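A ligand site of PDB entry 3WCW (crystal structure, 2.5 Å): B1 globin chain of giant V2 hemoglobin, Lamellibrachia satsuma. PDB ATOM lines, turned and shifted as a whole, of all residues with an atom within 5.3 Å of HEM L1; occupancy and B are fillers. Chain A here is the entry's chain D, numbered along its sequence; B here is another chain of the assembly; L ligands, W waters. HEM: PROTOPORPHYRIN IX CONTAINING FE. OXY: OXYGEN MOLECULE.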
ATOM      1  N   PHE A  37      14.187  18.543   6.696  1.00  0.00           N
ATOM      2  CA  PHE A  37      15.178  18.023   5.761  1.00  0.00           C
ATOM      3  C   PHE A  37      16.559  18.675   5.874  1.00  0.00           C
ATOM      4  O   PHE A  37      17.568  17.991   5.687  1.00  0.00           O
ATOM      5  CB  PHE A  37      14.631  18.093   4.346  1.00  0.00           C
ATOM      6  CG  PHE A  37      13.716  16.968   4.014  1.00  0.00           C
ATOM      7  CD1 PHE A  37      14.227  15.743   3.589  1.00  0.00           C
ATOM      8  CD2 PHE A  37      12.348  17.085   4.229  1.00  0.00           C
ATOM      9  CE1 PHE A  37      13.384  14.647   3.385  1.00  0.00           C
ATOM     10  CE2 PHE A  37      11.498  15.996   4.026  1.00  0.00           C
ATOM     11  CZ  PHE A  37      12.016  14.777   3.604  1.00  0.00           C
ATOM     12  N   LEU A  40      17.983  16.821   8.604  1.00  0.00           N
ATOM     13  CA  LEU A  40      18.318  15.445   8.251  1.00  0.00           C
ATOM     14  C   LEU A  40      19.657  15.438   7.521  1.00  0.00           C
ATOM     15  O   LEU A  40      20.496  14.563   7.726  1.00  0.00           O
ATOM     16  CB  LEU A  40      17.260  14.840   7.329  1.00  0.00           C
ATOM     17  CG  LEU A  40      17.614  13.408   6.923  1.00  0.00           C
ATOM     18  CD1 LEU A  40      17.516  12.505   8.133  1.00  0.00           C
ATOM     19  CD2 LEU A  40      16.694  12.926   5.817  1.00  0.00           C
ATOM     20  N   SER A  47      22.718  11.549   2.349  1.00  0.00           N
ATOM     21  CA  SER A  47      21.358  11.284   1.882  1.00  0.00           C
ATOM     22  C   SER A  47      20.808  12.431   1.016  1.00  0.00           C
ATOM     23  O   SER A  47      19.868  12.238   0.241  1.00  0.00           O
ATOM     24  CB  SER A  47      20.424  11.065   3.080  1.00  0.00           C
ATOM     25  OG  SER A  47      20.313  12.228   3.864  1.00  0.00           O
ATOM     26  N   LEU A  50      20.169  11.732  -2.550  1.00  0.00           N
ATOM     27  CA  LEU A  50      18.965  10.960  -2.824  1.00  0.00           C
ATOM     28  C   LEU A  50      17.781  11.823  -3.287  1.00  0.00           C
ATOM     29  O   LEU A  50      16.855  11.324  -3.913  1.00  0.00           O
ATOM     30  CB  LEU A  50      18.547  10.144  -1.590  1.00  0.00           C
ATOM     31  CG  LEU A  50      19.530   9.117  -1.021  1.00  0.00           C
ATOM     32  CD1 LEU A  50      18.932   8.467   0.211  1.00  0.00           C
ATOM     33  CD2 LEU A  50      19.839   8.058  -2.059  1.00  0.00           C
ATOM     34  N   PHE A  51      17.809  13.110  -2.965  1.00  0.00           N
ATOM     35  CA  PHE A  51      16.720  13.998  -3.329  1.00  0.00           C
ATOM     36  C   PHE A  51      16.979  14.841  -4.575  1.00  0.00           C
ATOM     37  O   PHE A  51      16.442  15.951  -4.706  1.00  0.00           O
ATOM     38  CB  PHE A  51      16.363  14.894  -2.137  1.00  0.00           C
ATOM     39  CG  PHE A  51      16.064  14.121  -0.890  1.00  0.00           C
ATOM     40  CD1 PHE A  51      17.069  13.852   0.047  1.00  0.00           C
ATOM     41  CD2 PHE A  51      14.792  13.580  -0.687  1.00  0.00           C
ATOM     42  CE1 PHE A  51      16.807  13.062   1.160  1.00  0.00           C
ATOM     43  CE2 PHE A  51      14.531  12.790   0.426  1.00  0.00           C
ATOM     44  CZ  PHE A  51      15.544  12.529   1.355  1.00  0.00           C
ATOM     45  N   ASN A  53      16.066  14.267  -7.835  1.00  0.00           N
ATOM     46  CA  ASN A  53      14.955  14.436  -8.764  1.00  0.00           C
ATOM     47  C   ASN A  53      13.930  15.478  -8.355  1.00  0.00           C
ATOM     48  O   ASN A  53      13.140  15.933  -9.186  1.00  0.00           O
ATOM     49  CB  ASN A  53      14.246  13.107  -9.037  1.00  0.00           C
ATOM     50  CG  ASN A  53      14.788  12.405 -10.268  1.00  0.00           C
ATOM     51  OD1 ASN A  53      15.934  11.952 -10.285  1.00  0.00           O
ATOM     52  ND2 ASN A  53      13.963  12.330 -11.314  1.00  0.00           N
ATOM     53  N   VAL A  54      13.938  15.869  -7.071  1.00  0.00           N
ATOM     54  CA  VAL A  54      13.018  16.884  -6.595  1.00  0.00           C
ATOM     55  C   VAL A  54      13.773  18.186  -6.323  1.00  0.00           C
ATOM     56  O   VAL A  54      13.372  19.004  -5.494  1.00  0.00           O
ATOM     57  CB  VAL A  54      12.257  16.434  -5.337  1.00  0.00           C
ATOM     58  CG1 VAL A  54      11.285  15.333  -5.711  1.00  0.00           C
ATOM     59  CG2 VAL A  54      13.234  15.979  -4.249  1.00  0.00           C
ATOM     60  N   HIS A  67       7.808  18.353  -2.645  1.00  0.00           N
ATOM     61  CA  HIS A  67       8.261  17.090  -2.074  1.00  0.00           C
ATOM     62  C   HIS A  67       7.954  17.053  -0.570  1.00  0.00           C
ATOM     63  O   HIS A  67       7.284  16.134  -0.087  1.00  0.00           O
ATOM     64  CB  HIS A  67       9.753  16.879  -2.287  1.00  0.00           C
ATOM     65  CG  HIS A  67      10.295  15.681  -1.568  1.00  0.00           C
ATOM     66  ND1 HIS A  67       9.931  14.393  -1.886  1.00  0.00           N
ATOM     67  CD2 HIS A  67      11.119  15.597  -0.496  1.00  0.00           C
ATOM     68  CE1 HIS A  67      10.507  13.556  -1.041  1.00  0.00           C
ATOM     69  NE2 HIS A  67      11.233  14.263  -0.185  1.00  0.00           N
ATOM     70  N   ARG A  70       4.464  16.833   0.326  1.00  0.00           N
ATOM     71  CA  ARG A  70       4.068  15.456   0.087  1.00  0.00           C
ATOM     72  C   ARG A  70       4.464  14.532   1.253  1.00  0.00           C
ATOM     73  O   ARG A  70       3.725  13.601   1.602  1.00  0.00           O
ATOM     74  CB  ARG A  70       4.718  15.006  -1.210  1.00  0.00           C
ATOM     75  CG  ARG A  70       3.976  13.981  -2.016  1.00  0.00           C
ATOM     76  CD  ARG A  70       4.691  13.773  -3.375  1.00  0.00           C
ATOM     77  NE  ARG A  70       4.616  14.975  -4.196  1.00  0.00           N
ATOM     78  CZ  ARG A  70       5.636  15.469  -4.891  1.00  0.00           C
ATOM     79  NH1 ARG A  70       6.826  14.878  -4.871  1.00  0.00           N
ATOM     80  NH2 ARG A  70       5.456  16.573  -5.622  1.00  0.00           N
ATOM     81  N   VAL A  71       5.626  14.787   1.851  1.00  0.00           N
ATOM     82  CA  VAL A  71       6.119  13.963   2.957  1.00  0.00           C
ATOM     83  C   VAL A  71       5.346  14.236   4.253  1.00  0.00           C
ATOM     84  O   VAL A  71       4.928  13.309   4.968  1.00  0.00           O
ATOM     85  CB  VAL A  71       7.641  14.232   3.206  1.00  0.00           C
ATOM     86  CG1 VAL A  71       8.113  13.526   4.471  1.00  0.00           C
ATOM     87  CG2 VAL A  71       8.454  13.762   1.984  1.00  0.00           C
ATOM     88  N   GLY A  74       2.164  12.543   4.100  1.00  0.00           N
ATOM     89  CA  GLY A  74       2.198  11.119   4.393  1.00  0.00           C
ATOM     90  C   GLY A  74       2.221  10.923   5.898  1.00  0.00           C
ATOM     91  O   GLY A  74       1.499  10.093   6.457  1.00  0.00           O
ATOM     92  N   LEU A  75       3.078  11.696   6.567  1.00  0.00           N
ATOM     93  CA  LEU A  75       3.207  11.619   8.017  1.00  0.00           C
ATOM     94  C   LEU A  75       1.820  11.890   8.606  1.00  0.00           C
ATOM     95  O   LEU A  75       1.395  11.225   9.543  1.00  0.00           O
ATOM     96  CB  LEU A  75       4.203  12.687   8.490  1.00  0.00           C
ATOM     97  CG  LEU A  75       4.649  12.685   9.940  1.00  0.00           C
ATOM     98  CD1 LEU A  75       5.360  11.380  10.262  1.00  0.00           C
ATOM     99  CD2 LEU A  75       5.592  13.848  10.160  1.00  0.00           C
ATOM    100  N   LEU A  95       3.934   2.971   1.708  1.00  0.00           N
ATOM    101  CA  LEU A  95       5.002   3.936   1.939  1.00  0.00           C
ATOM    102  C   LEU A  95       6.366   3.254   1.864  1.00  0.00           C
ATOM    103  O   LEU A  95       7.331   3.810   1.332  1.00  0.00           O
ATOM    104  CB  LEU A  95       4.836   4.600   3.316  1.00  0.00           C
ATOM    105  CG  LEU A  95       3.890   5.796   3.346  1.00  0.00           C
ATOM    106  CD1 LEU A  95       3.711   6.328   4.765  1.00  0.00           C
ATOM    107  CD2 LEU A  95       4.462   6.862   2.442  1.00  0.00           C
ATOM    108  N   GLN A  98       7.412   2.642  -1.621  1.00  0.00           N
ATOM    109  CA  GLN A  98       7.848   3.882  -2.243  1.00  0.00           C
ATOM    110  C   GLN A  98       9.265   4.277  -1.834  1.00  0.00           C
ATOM    111  O   GLN A  98       9.896   5.123  -2.482  1.00  0.00           O
ATOM    112  CB  GLN A  98       6.884   5.022  -1.908  1.00  0.00           C
ATOM    113  CG  GLN A  98       5.483   4.819  -2.490  1.00  0.00           C
ATOM    114  CD  GLN A  98       4.515   5.921  -2.081  1.00  0.00           C
ATOM    115  OE1 GLN A  98       4.353   6.201  -0.903  1.00  0.00           O
ATOM    116  NE2 GLN A  98       3.865   6.536  -3.067  1.00  0.00           N
ATOM    117  N   HIS A  99       9.774   3.678  -0.757  1.00  0.00           N
ATOM    118  CA  HIS A  99      11.120   4.027  -0.335  1.00  0.00           C
ATOM    119  C   HIS A  99      12.160   2.995  -0.730  1.00  0.00           C
ATOM    120  O   HIS A  99      13.243   3.353  -1.190  1.00  0.00           O
ATOM    121  CB  HIS A  99      11.164   4.286   1.181  1.00  0.00           C
ATOM    122  CG  HIS A  99      10.637   5.633   1.559  1.00  0.00           C
ATOM    123  ND1 HIS A  99       9.288   5.906   1.688  1.00  0.00           N
ATOM    124  CD2 HIS A  99      11.276   6.811   1.759  1.00  0.00           C
ATOM    125  CE1 HIS A  99       9.121   7.188   1.936  1.00  0.00           C
ATOM    126  NE2 HIS A  99      10.304   7.765   1.989  1.00  0.00           N
ATOM    127  N   ARG A 102      13.841   3.418  -3.934  1.00  0.00           N
ATOM    128  CA  ARG A 102      14.889   4.421  -4.016  1.00  0.00           C
ATOM    129  C   ARG A 102      16.222   3.824  -3.570  1.00  0.00           C
ATOM    130  O   ARG A 102      16.506   3.738  -2.373  1.00  0.00           O
ATOM    131  CB  ARG A 102      14.547   5.630  -3.134  1.00  0.00           C
ATOM    132  CG  ARG A 102      13.118   6.163  -3.296  1.00  0.00           C
ATOM    133  CD  ARG A 102      12.826   6.684  -4.695  1.00  0.00           C
ATOM    134  NE  ARG A 102      13.789   7.703  -5.113  1.00  0.00           N
ATOM    135  CZ  ARG A 102      13.621   8.545  -6.129  1.00  0.00           C
ATOM    136  NH1 ARG A 102      12.502   8.500  -6.860  1.00  0.00           N
ATOM    137  NH2 ARG A 102      14.550   9.441  -6.413  1.00  0.00           N
ATOM    138  N   LEU A 105      18.816   4.310  -0.104  1.00  0.00           N
ATOM    139  CA  LEU A 105      18.107   4.550   1.149  1.00  0.00           C
ATOM    140  C   LEU A 105      18.464   3.544   2.221  1.00  0.00           C
ATOM    141  O   LEU A 105      18.094   2.360   2.142  1.00  0.00           O
ATOM    142  CB  LEU A 105      16.603   4.500   0.921  1.00  0.00           C
ATOM    143  CG  LEU A 105      15.852   5.656   1.561  1.00  0.00           C
ATOM    144  CD1 LEU A 105      16.169   6.948   0.803  1.00  0.00           C
ATOM    145  CD2 LEU A 105      14.369   5.389   1.534  1.00  0.00           C
ATOM    146  N   TYR A 109      19.002   5.907   7.911  1.00  0.00           N
ATOM    147  CA  TYR A 109      18.599   7.259   7.562  1.00  0.00           C
ATOM    148  C   TYR A 109      17.248   7.554   8.190  1.00  0.00           C
ATOM    149  O   TYR A 109      16.947   8.699   8.547  1.00  0.00           O
ATOM    150  CB  TYR A 109      18.495   7.431   6.043  1.00  0.00           C
ATOM    151  CG  TYR A 109      19.815   7.371   5.298  1.00  0.00           C
ATOM    152  CD1 TYR A 109      21.028   7.661   5.940  1.00  0.00           C
ATOM    153  CD2 TYR A 109      19.844   7.059   3.943  1.00  0.00           C
ATOM    154  CE1 TYR A 109      22.243   7.642   5.225  1.00  0.00           C
ATOM    155  CE2 TYR A 109      21.037   7.036   3.225  1.00  0.00           C
ATOM    156  CZ  TYR A 109      22.230   7.336   3.866  1.00  0.00           C
ATOM    157  OH  TYR A 109      23.405   7.338   3.141  1.00  0.00           O
ATOM    158  N   PHE A 110      16.420   6.516   8.320  1.00  0.00           N
ATOM    159  CA  PHE A 110      15.103   6.672   8.931  1.00  0.00           C
ATOM    160  C   PHE A 110      15.211   6.921  10.431  1.00  0.00           C
ATOM    161  O   PHE A 110      14.322   7.518  11.024  1.00  0.00           O
ATOM    162  CB  PHE A 110      14.234   5.445   8.674  1.00  0.00           C
ATOM    163  CG  PHE A 110      13.271   5.632   7.538  1.00  0.00           C
ATOM    164  CD1 PHE A 110      13.733   5.666   6.225  1.00  0.00           C
ATOM    165  CD2 PHE A 110      11.920   5.850   7.778  1.00  0.00           C
ATOM    166  CE1 PHE A 110      12.851   5.921   5.165  1.00  0.00           C
ATOM    167  CE2 PHE A 110      11.045   6.110   6.730  1.00  0.00           C
ATOM    168  CZ  PHE A 110      11.515   6.149   5.419  1.00  0.00           C
ATOM    169  N   MET A 113      15.924  10.579  10.824  1.00  0.00           N
ATOM    170  CA  MET A 113      14.693  11.365  10.648  1.00  0.00           C
ATOM    171  C   MET A 113      13.944  11.342  11.983  1.00  0.00           C
ATOM    172  O   MET A 113      13.420  12.369  12.444  1.00  0.00           O
ATOM    173  CB  MET A 113      13.832  10.779   9.525  1.00  0.00           C
ATOM    174  CG  MET A 113      12.492  11.490   9.248  1.00  0.00           C
ATOM    175  SD  MET A 113      12.563  13.194   8.555  1.00  0.00           S
ATOM    176  CE  MET A 113      12.433  12.876   6.862  1.00  0.00           C
ATOM    177  N   LEU A 117      12.710  14.605  13.969  1.00  0.00           N
ATOM    178  CA  LEU A 117      11.351  14.954  14.340  1.00  0.00           C
ATOM    179  C   LEU A 117      11.280  15.199  15.841  1.00  0.00           C
ATOM    180  O   LEU A 117      10.718  16.200  16.281  1.00  0.00           O
ATOM    181  CB  LEU A 117      10.383  13.852  13.905  1.00  0.00           C
ATOM    182  CG  LEU A 117      10.221  13.730  12.386  1.00  0.00           C
ATOM    183  CD1 LEU A 117       9.318  12.567  12.026  1.00  0.00           C
ATOM    184  CD2 LEU A 117       9.651  15.039  11.833  1.00  0.00           C
ATOM    185  N   LYS A 141       7.814   4.342  12.028  1.00  0.00           N
ATOM    186  CA  LYS A 141       9.140   4.383  11.441  1.00  0.00           C
ATOM    187  C   LYS A 141       9.643   3.007  11.044  1.00  0.00           C
ATOM    188  O   LYS A 141      10.142   2.835   9.937  1.00  0.00           O
ATOM    189  CB  LYS A 141      10.111   5.067  12.412  1.00  0.00           C
ATOM    190  CG  LYS A 141      11.473   5.437  11.810  1.00  0.00           C
ATOM    191  CD  LYS A 141      12.566   4.486  12.285  1.00  0.00           C
ATOM    192  CE  LYS A 141      12.818   4.619  13.775  1.00  0.00           C
ATOM    193  NZ  LYS A 141      13.735   3.556  14.308  1.00  0.00           N
ATOM    194  N   ILE A 144       7.723   1.748   7.953  1.00  0.00           N
ATOM    195  CA  ILE A 144       7.991   2.444   6.706  1.00  0.00           C
ATOM    196  C   ILE A 144       9.385   2.093   6.173  1.00  0.00           C
ATOM    197  O   ILE A 144       9.607   2.046   4.971  1.00  0.00           O
ATOM    198  CB  ILE A 144       7.885   3.981   6.863  1.00  0.00           C
ATOM    199  CG1 ILE A 144       6.428   4.363   7.170  1.00  0.00           C
ATOM    200  CG2 ILE A 144       8.356   4.689   5.600  1.00  0.00           C
ATOM    201  CD1 ILE A 144       6.211   5.875   7.330  1.00  0.00           C
ATOM    202  N   HIS B  89       3.514  15.575 -10.584  1.00  0.00           N
ATOM    203  CA  HIS B  89       3.889  14.358  -9.867  1.00  0.00           C
ATOM    204  C   HIS B  89       2.685  13.411  -9.892  1.00  0.00           C
ATOM    205  O   HIS B  89       2.825  12.209 -10.125  1.00  0.00           O
ATOM    206  CB  HIS B  89       4.263  14.700  -8.419  1.00  0.00           C
ATOM    207  CG  HIS B  89       4.775  13.534  -7.635  1.00  0.00           C
ATOM    208  ND1 HIS B  89       6.100  13.136  -7.660  1.00  0.00           N
ATOM    209  CD2 HIS B  89       4.156  12.685  -6.790  1.00  0.00           C
ATOM    210  CE1 HIS B  89       6.261  12.087  -6.878  1.00  0.00           C
ATOM    211  NE2 HIS B  89       5.093  11.790  -6.331  1.00  0.00           N
ATOM    212  N   GLN B  93       1.779   9.690 -11.949  1.00  0.00           N
ATOM    213  CA  GLN B  93       1.257   8.475 -11.361  1.00  0.00           C
ATOM    214  C   GLN B  93      -0.037   8.033 -12.035  1.00  0.00           C
ATOM    215  O   GLN B  93      -0.341   6.846 -12.067  1.00  0.00           O
ATOM    216  CB  GLN B  93       1.013   8.657  -9.853  1.00  0.00           C
ATOM    217  CG  GLN B  93       2.287   8.835  -9.075  1.00  0.00           C
ATOM    218  CD  GLN B  93       2.058   9.352  -7.665  1.00  0.00           C
ATOM    219  OE1 GLN B  93       1.413  10.383  -7.474  1.00  0.00           O
ATOM    220  NE2 GLN B  93       2.602   8.639  -6.682  1.00  0.00           N
HETATM  221  CHA HEM L   1       9.471  10.171  -1.089  1.00  0.00           C
HETATM  222  CHB HEM L   1       7.224  10.164   3.115  1.00  0.00           C
HETATM  223  CHC HEM L   1      11.422   9.581   5.436  1.00  0.00           C
HETATM  224  CHD HEM L   1      13.673   9.520   1.176  1.00  0.00           C
HETATM  225  C1A HEM L   1       8.464  10.224  -0.147  1.00  0.00           C
HETATM  226  C2A HEM L   1       7.113  10.414  -0.470  1.00  0.00           C
HETATM  227  C3A HEM L   1       6.450  10.403   0.712  1.00  0.00           C
HETATM  228  C4A HEM L   1       7.431  10.211   1.798  1.00  0.00           C
HETATM  229  CMA HEM L   1       4.938  10.572   0.924  1.00  0.00           C
HETATM  230  CAA HEM L   1       6.505  10.598  -1.845  1.00  0.00           C
HETATM  231  CBA HEM L   1       5.897   9.366  -2.415  1.00  0.00           C
HETATM  232  CGA HEM L   1       5.301   9.574  -3.805  1.00  0.00           C
HETATM  233  O1A HEM L   1       6.005   9.348  -4.809  1.00  0.00           O
HETATM  234  O2A HEM L   1       4.185   9.975  -3.890  1.00  0.00           O
HETATM  235  C1B HEM L   1       8.161  10.005   4.172  1.00  0.00           C
HETATM  236  C2B HEM L   1       7.808   9.995   5.584  1.00  0.00           C
HETATM  237  C3B HEM L   1       9.076   9.832   6.264  1.00  0.00           C
HETATM  238  C4B HEM L   1      10.045   9.749   5.218  1.00  0.00           C
HETATM  239  CMB HEM L   1       6.446  10.131   6.176  1.00  0.00           C
HETATM  240  CAB HEM L   1       9.201   9.777   7.709  1.00  0.00           C
HETATM  241  CBB HEM L   1       9.473   8.689   8.392  1.00  0.00           C
HETATM  242  C1C HEM L   1      12.394   9.504   4.454  1.00  0.00           C
HETATM  243  C2C HEM L   1      13.825   9.327   4.778  1.00  0.00           C
HETATM  244  C3C HEM L   1      14.530   9.301   3.551  1.00  0.00           C
HETATM  245  C4C HEM L   1      13.422   9.474   2.509  1.00  0.00           C
HETATM  246  CMC HEM L   1      14.402   9.205   6.185  1.00  0.00           C
HETATM  247  CAC HEM L   1      15.858   9.162   3.357  1.00  0.00           C
HETATM  248  CBC HEM L   1      16.919   9.886   3.306  1.00  0.00           C
HETATM  249  C1D HEM L   1      12.719   9.697   0.173  1.00  0.00           C
HETATM  250  C2D HEM L   1      13.055   9.754  -1.303  1.00  0.00           C
HETATM  251  C3D HEM L   1      11.849   9.946  -1.918  1.00  0.00           C
HETATM  252  C4D HEM L   1      10.817   9.988  -0.858  1.00  0.00           C
HETATM  253  CMD HEM L   1      14.467   9.632  -1.886  1.00  0.00           C
HETATM  254  CAD HEM L   1      11.603  10.089  -3.408  1.00  0.00           C
HETATM  255  CBD HEM L   1      11.734  11.525  -3.855  1.00  0.00           C
HETATM  256  CGD HEM L   1      11.497  11.709  -5.304  1.00  0.00           C
HETATM  257  O1D HEM L   1      10.319  11.581  -5.781  1.00  0.00           O
HETATM  258  O2D HEM L   1      12.481  11.999  -6.048  1.00  0.00           O
HETATM  259  NA  HEM L   1       8.677  10.094   1.239  1.00  0.00           N
HETATM  260  NB  HEM L   1       9.464   9.865   3.933  1.00  0.00           N
HETATM  261  NC  HEM L   1      12.202   9.586   3.080  1.00  0.00           N
HETATM  262  ND  HEM L   1      11.390   9.834   0.377  1.00  0.00           N
HETATM  263 FE   HEM L   1      10.435   9.830   2.157  1.00  0.00          FE
HETATM  264  O1  OXY L   2      10.569  11.617   2.293  1.00  0.00           O
HETATM  265  O2  OXY L   2      11.601  12.248   2.095  1.00  0.00           O
HETATM  266  CHA HEM L   3      -3.801   6.566  -7.182  1.00  0.00           C
HETATM  267  CHB HEM L   3      -4.905  11.077  -6.180  1.00  0.00           C
HETATM  268  CHC HEM L   3      -8.456  10.976  -9.418  1.00  0.00           C
HETATM  269  CHD HEM L   3      -7.296   6.436 -10.451  1.00  0.00           C
HETATM  270  C1A HEM L   3      -3.786   7.808  -6.603  1.00  0.00           C
HETATM  271  C2A HEM L   3      -2.894   8.176  -5.588  1.00  0.00           C
HETATM  272  C3A HEM L   3      -3.193   9.460  -5.292  1.00  0.00           C
HETATM  273  C4A HEM L   3      -4.291   9.888  -6.152  1.00  0.00           C
HETATM  274  CMA HEM L   3      -2.517  10.346  -4.246  1.00  0.00           C
HETATM  275  CAA HEM L   3      -1.824   7.314  -4.952  1.00  0.00           C
HETATM  276  CBA HEM L   3      -0.466   7.540  -5.566  1.00  0.00           C
HETATM  277  CGA HEM L   3       0.626   6.673  -4.949  1.00  0.00           C
HETATM  278  O1A HEM L   3       1.198   5.808  -5.657  1.00  0.00           O
HETATM  279  O2A HEM L   3       0.887   6.833  -3.792  1.00  0.00           O
HETATM  280  C1B HEM L   3      -5.982  11.490  -6.979  1.00  0.00           C
HETATM  281  C2B HEM L   3      -6.580  12.809  -6.914  1.00  0.00           C
HETATM  282  C3B HEM L   3      -7.642  12.763  -7.887  1.00  0.00           C
HETATM  283  C4B HEM L   3      -7.584  11.447  -8.433  1.00  0.00           C
HETATM  284  CMB HEM L   3      -6.180  13.947  -6.038  1.00  0.00           C
HETATM  285  CAB HEM L   3      -8.531  13.878  -8.158  1.00  0.00           C
HETATM  286  CBB HEM L   3      -8.212  14.964  -8.817  1.00  0.00           C
HETATM  287  C1C HEM L   3      -8.439   9.718  -9.976  1.00  0.00           C
HETATM  288  C2C HEM L   3      -9.401   9.297 -11.011  1.00  0.00           C
HETATM  289  C3C HEM L   3      -9.089   7.977 -11.344  1.00  0.00           C
HETATM  290  C4C HEM L   3      -7.909   7.649 -10.453  1.00  0.00           C
HETATM  291  CMC HEM L   3     -10.524  10.161 -11.601  1.00  0.00           C
HETATM  292  CAC HEM L   3      -9.715   7.176 -12.252  1.00  0.00           C
HETATM  293  CBC HEM L   3     -10.738   6.393 -12.313  1.00  0.00           C
HETATM  294  C1D HEM L   3      -6.228   6.069  -9.653  1.00  0.00           C
HETATM  295  C2D HEM L   3      -5.597   4.695  -9.685  1.00  0.00           C
HETATM  296  C3D HEM L   3      -4.594   4.760  -8.735  1.00  0.00           C
HETATM  297  C4D HEM L   3      -4.634   6.127  -8.166  1.00  0.00           C
HETATM  298  CMD HEM L   3      -6.043   3.562 -10.596  1.00  0.00           C
HETATM  299  CAD HEM L   3      -3.620   3.669  -8.326  1.00  0.00           C
HETATM  300  CBD HEM L   3      -4.120   2.814  -7.202  1.00  0.00           C
HETATM  301  CGD HEM L   3      -3.154   1.782  -6.790  1.00  0.00           C
HETATM  302  O1D HEM L   3      -3.261   0.598  -7.202  1.00  0.00           O
HETATM  303  O2D HEM L   3      -2.239   2.109  -6.019  1.00  0.00           O
HETATM  304  NA  HEM L   3      -4.656   8.847  -6.961  1.00  0.00           N
HETATM  305  NB  HEM L   3      -6.548  10.670  -7.864  1.00  0.00           N
HETATM  306  NC  HEM L   3      -7.571   8.686  -9.678  1.00  0.00           N
HETATM  307  ND  HEM L   3      -5.623   6.866  -8.748  1.00  0.00           N
HETATM  308 FE   HEM L   3      -6.091   8.760  -8.334  1.00  0.00          FE
HETATM  309  O   HOH W   1       8.559  12.885  -3.859  1.00  0.00           O
HETATM  310  O   HOH W   2       1.149  11.389  -4.897  1.00  0.00           O
HETATM  311  O   HOH W   3       2.180  10.600  -1.765  1.00  0.00           O
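FE of HEM L1 is bound by NE2 of His 99 (2.1 Å).
A ring nitrogen (NE2) of His 89 of chain B is in hydrogen-bond range of an oxygen (O1A) of HEM L1, at 3.0 Å.
An oxygen (O2D) of HEM L1 lies within salt-bridge range of the guanidinium group (NH2) of Arg 102 (3.3 Å).
O2A of HEM L1 lies within hydrogen-bond range of NE2 of Gln 93 of chain B (3.5 Å).
A ring nitrogen (NE2) of His 67 is in hydrogen-bond range of an oxygen (O2) of OXY L2, 3.1 Å away.
NE2 of Gln 98 lies within hydrogen-bond range of O2A of HEM L3, 3.1 Å away.
The side-chain amide nitrogen (NE2) of Gln 93 of chain B lies close to an oxygen (O1A) of HEM L3 (3.3 Å).
An iron atom (FE) of HEM L1 is bound by an oxygen (O1) of OXY L2 (1.8 Å).
ND1 of His 99 sits at hydrogen-bond distance from O of Leu 95 (2.9 Å).
The guanidinium group (NH1) of Arg 70 is in hydrogen-bond range of a ring nitrogen (ND1) of His 89 of chain B, 3.4 Å away.
Merely in contact with HEM L1: Arg 70 (3.3 Å), Leu 105 (3.4 Å), Phe 110 (3.4 Å), Gln 98 (3.4 Å), Phe 51 (3.5 Å), Tyr 109 (3.5 Å), Val 71 (3.5 Å), His 67 (3.5 Å), Val 54 (3.6 Å), Leu 50 (3.6 Å), Asn 53 (3.6 Å), Ser 47 (3.7 Å), Met 113 (3.7 Å), Leu 75 (3.7 Å) and Leu 40 (3.9 Å).
Hydrophobic or aromatic side chains within 4 Å of HEM L1: Leu 40, Leu 50, Phe 51, Val 54, His 67, Val 71, His 99, Leu 105, Phe 110, Met 113 and His 89 of chain B.
Of the 25 residues printed, 19 come within 4 Å of HEM L1.
The nearest printed residue that does not touch HEM L1 is Leu 95 (4.04 Å).
Water W1 lies within hydrogen-bond range of NH1 of Arg 70 (2.8 Å), ND1 of His 67 (2.8 Å) and O1D of HEM L1 (2.9 Å).
Water W2 bridges OE1 of Gln 93 of chain B (2.8 Å) and O2A of HEM L1 (3.5 Å).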
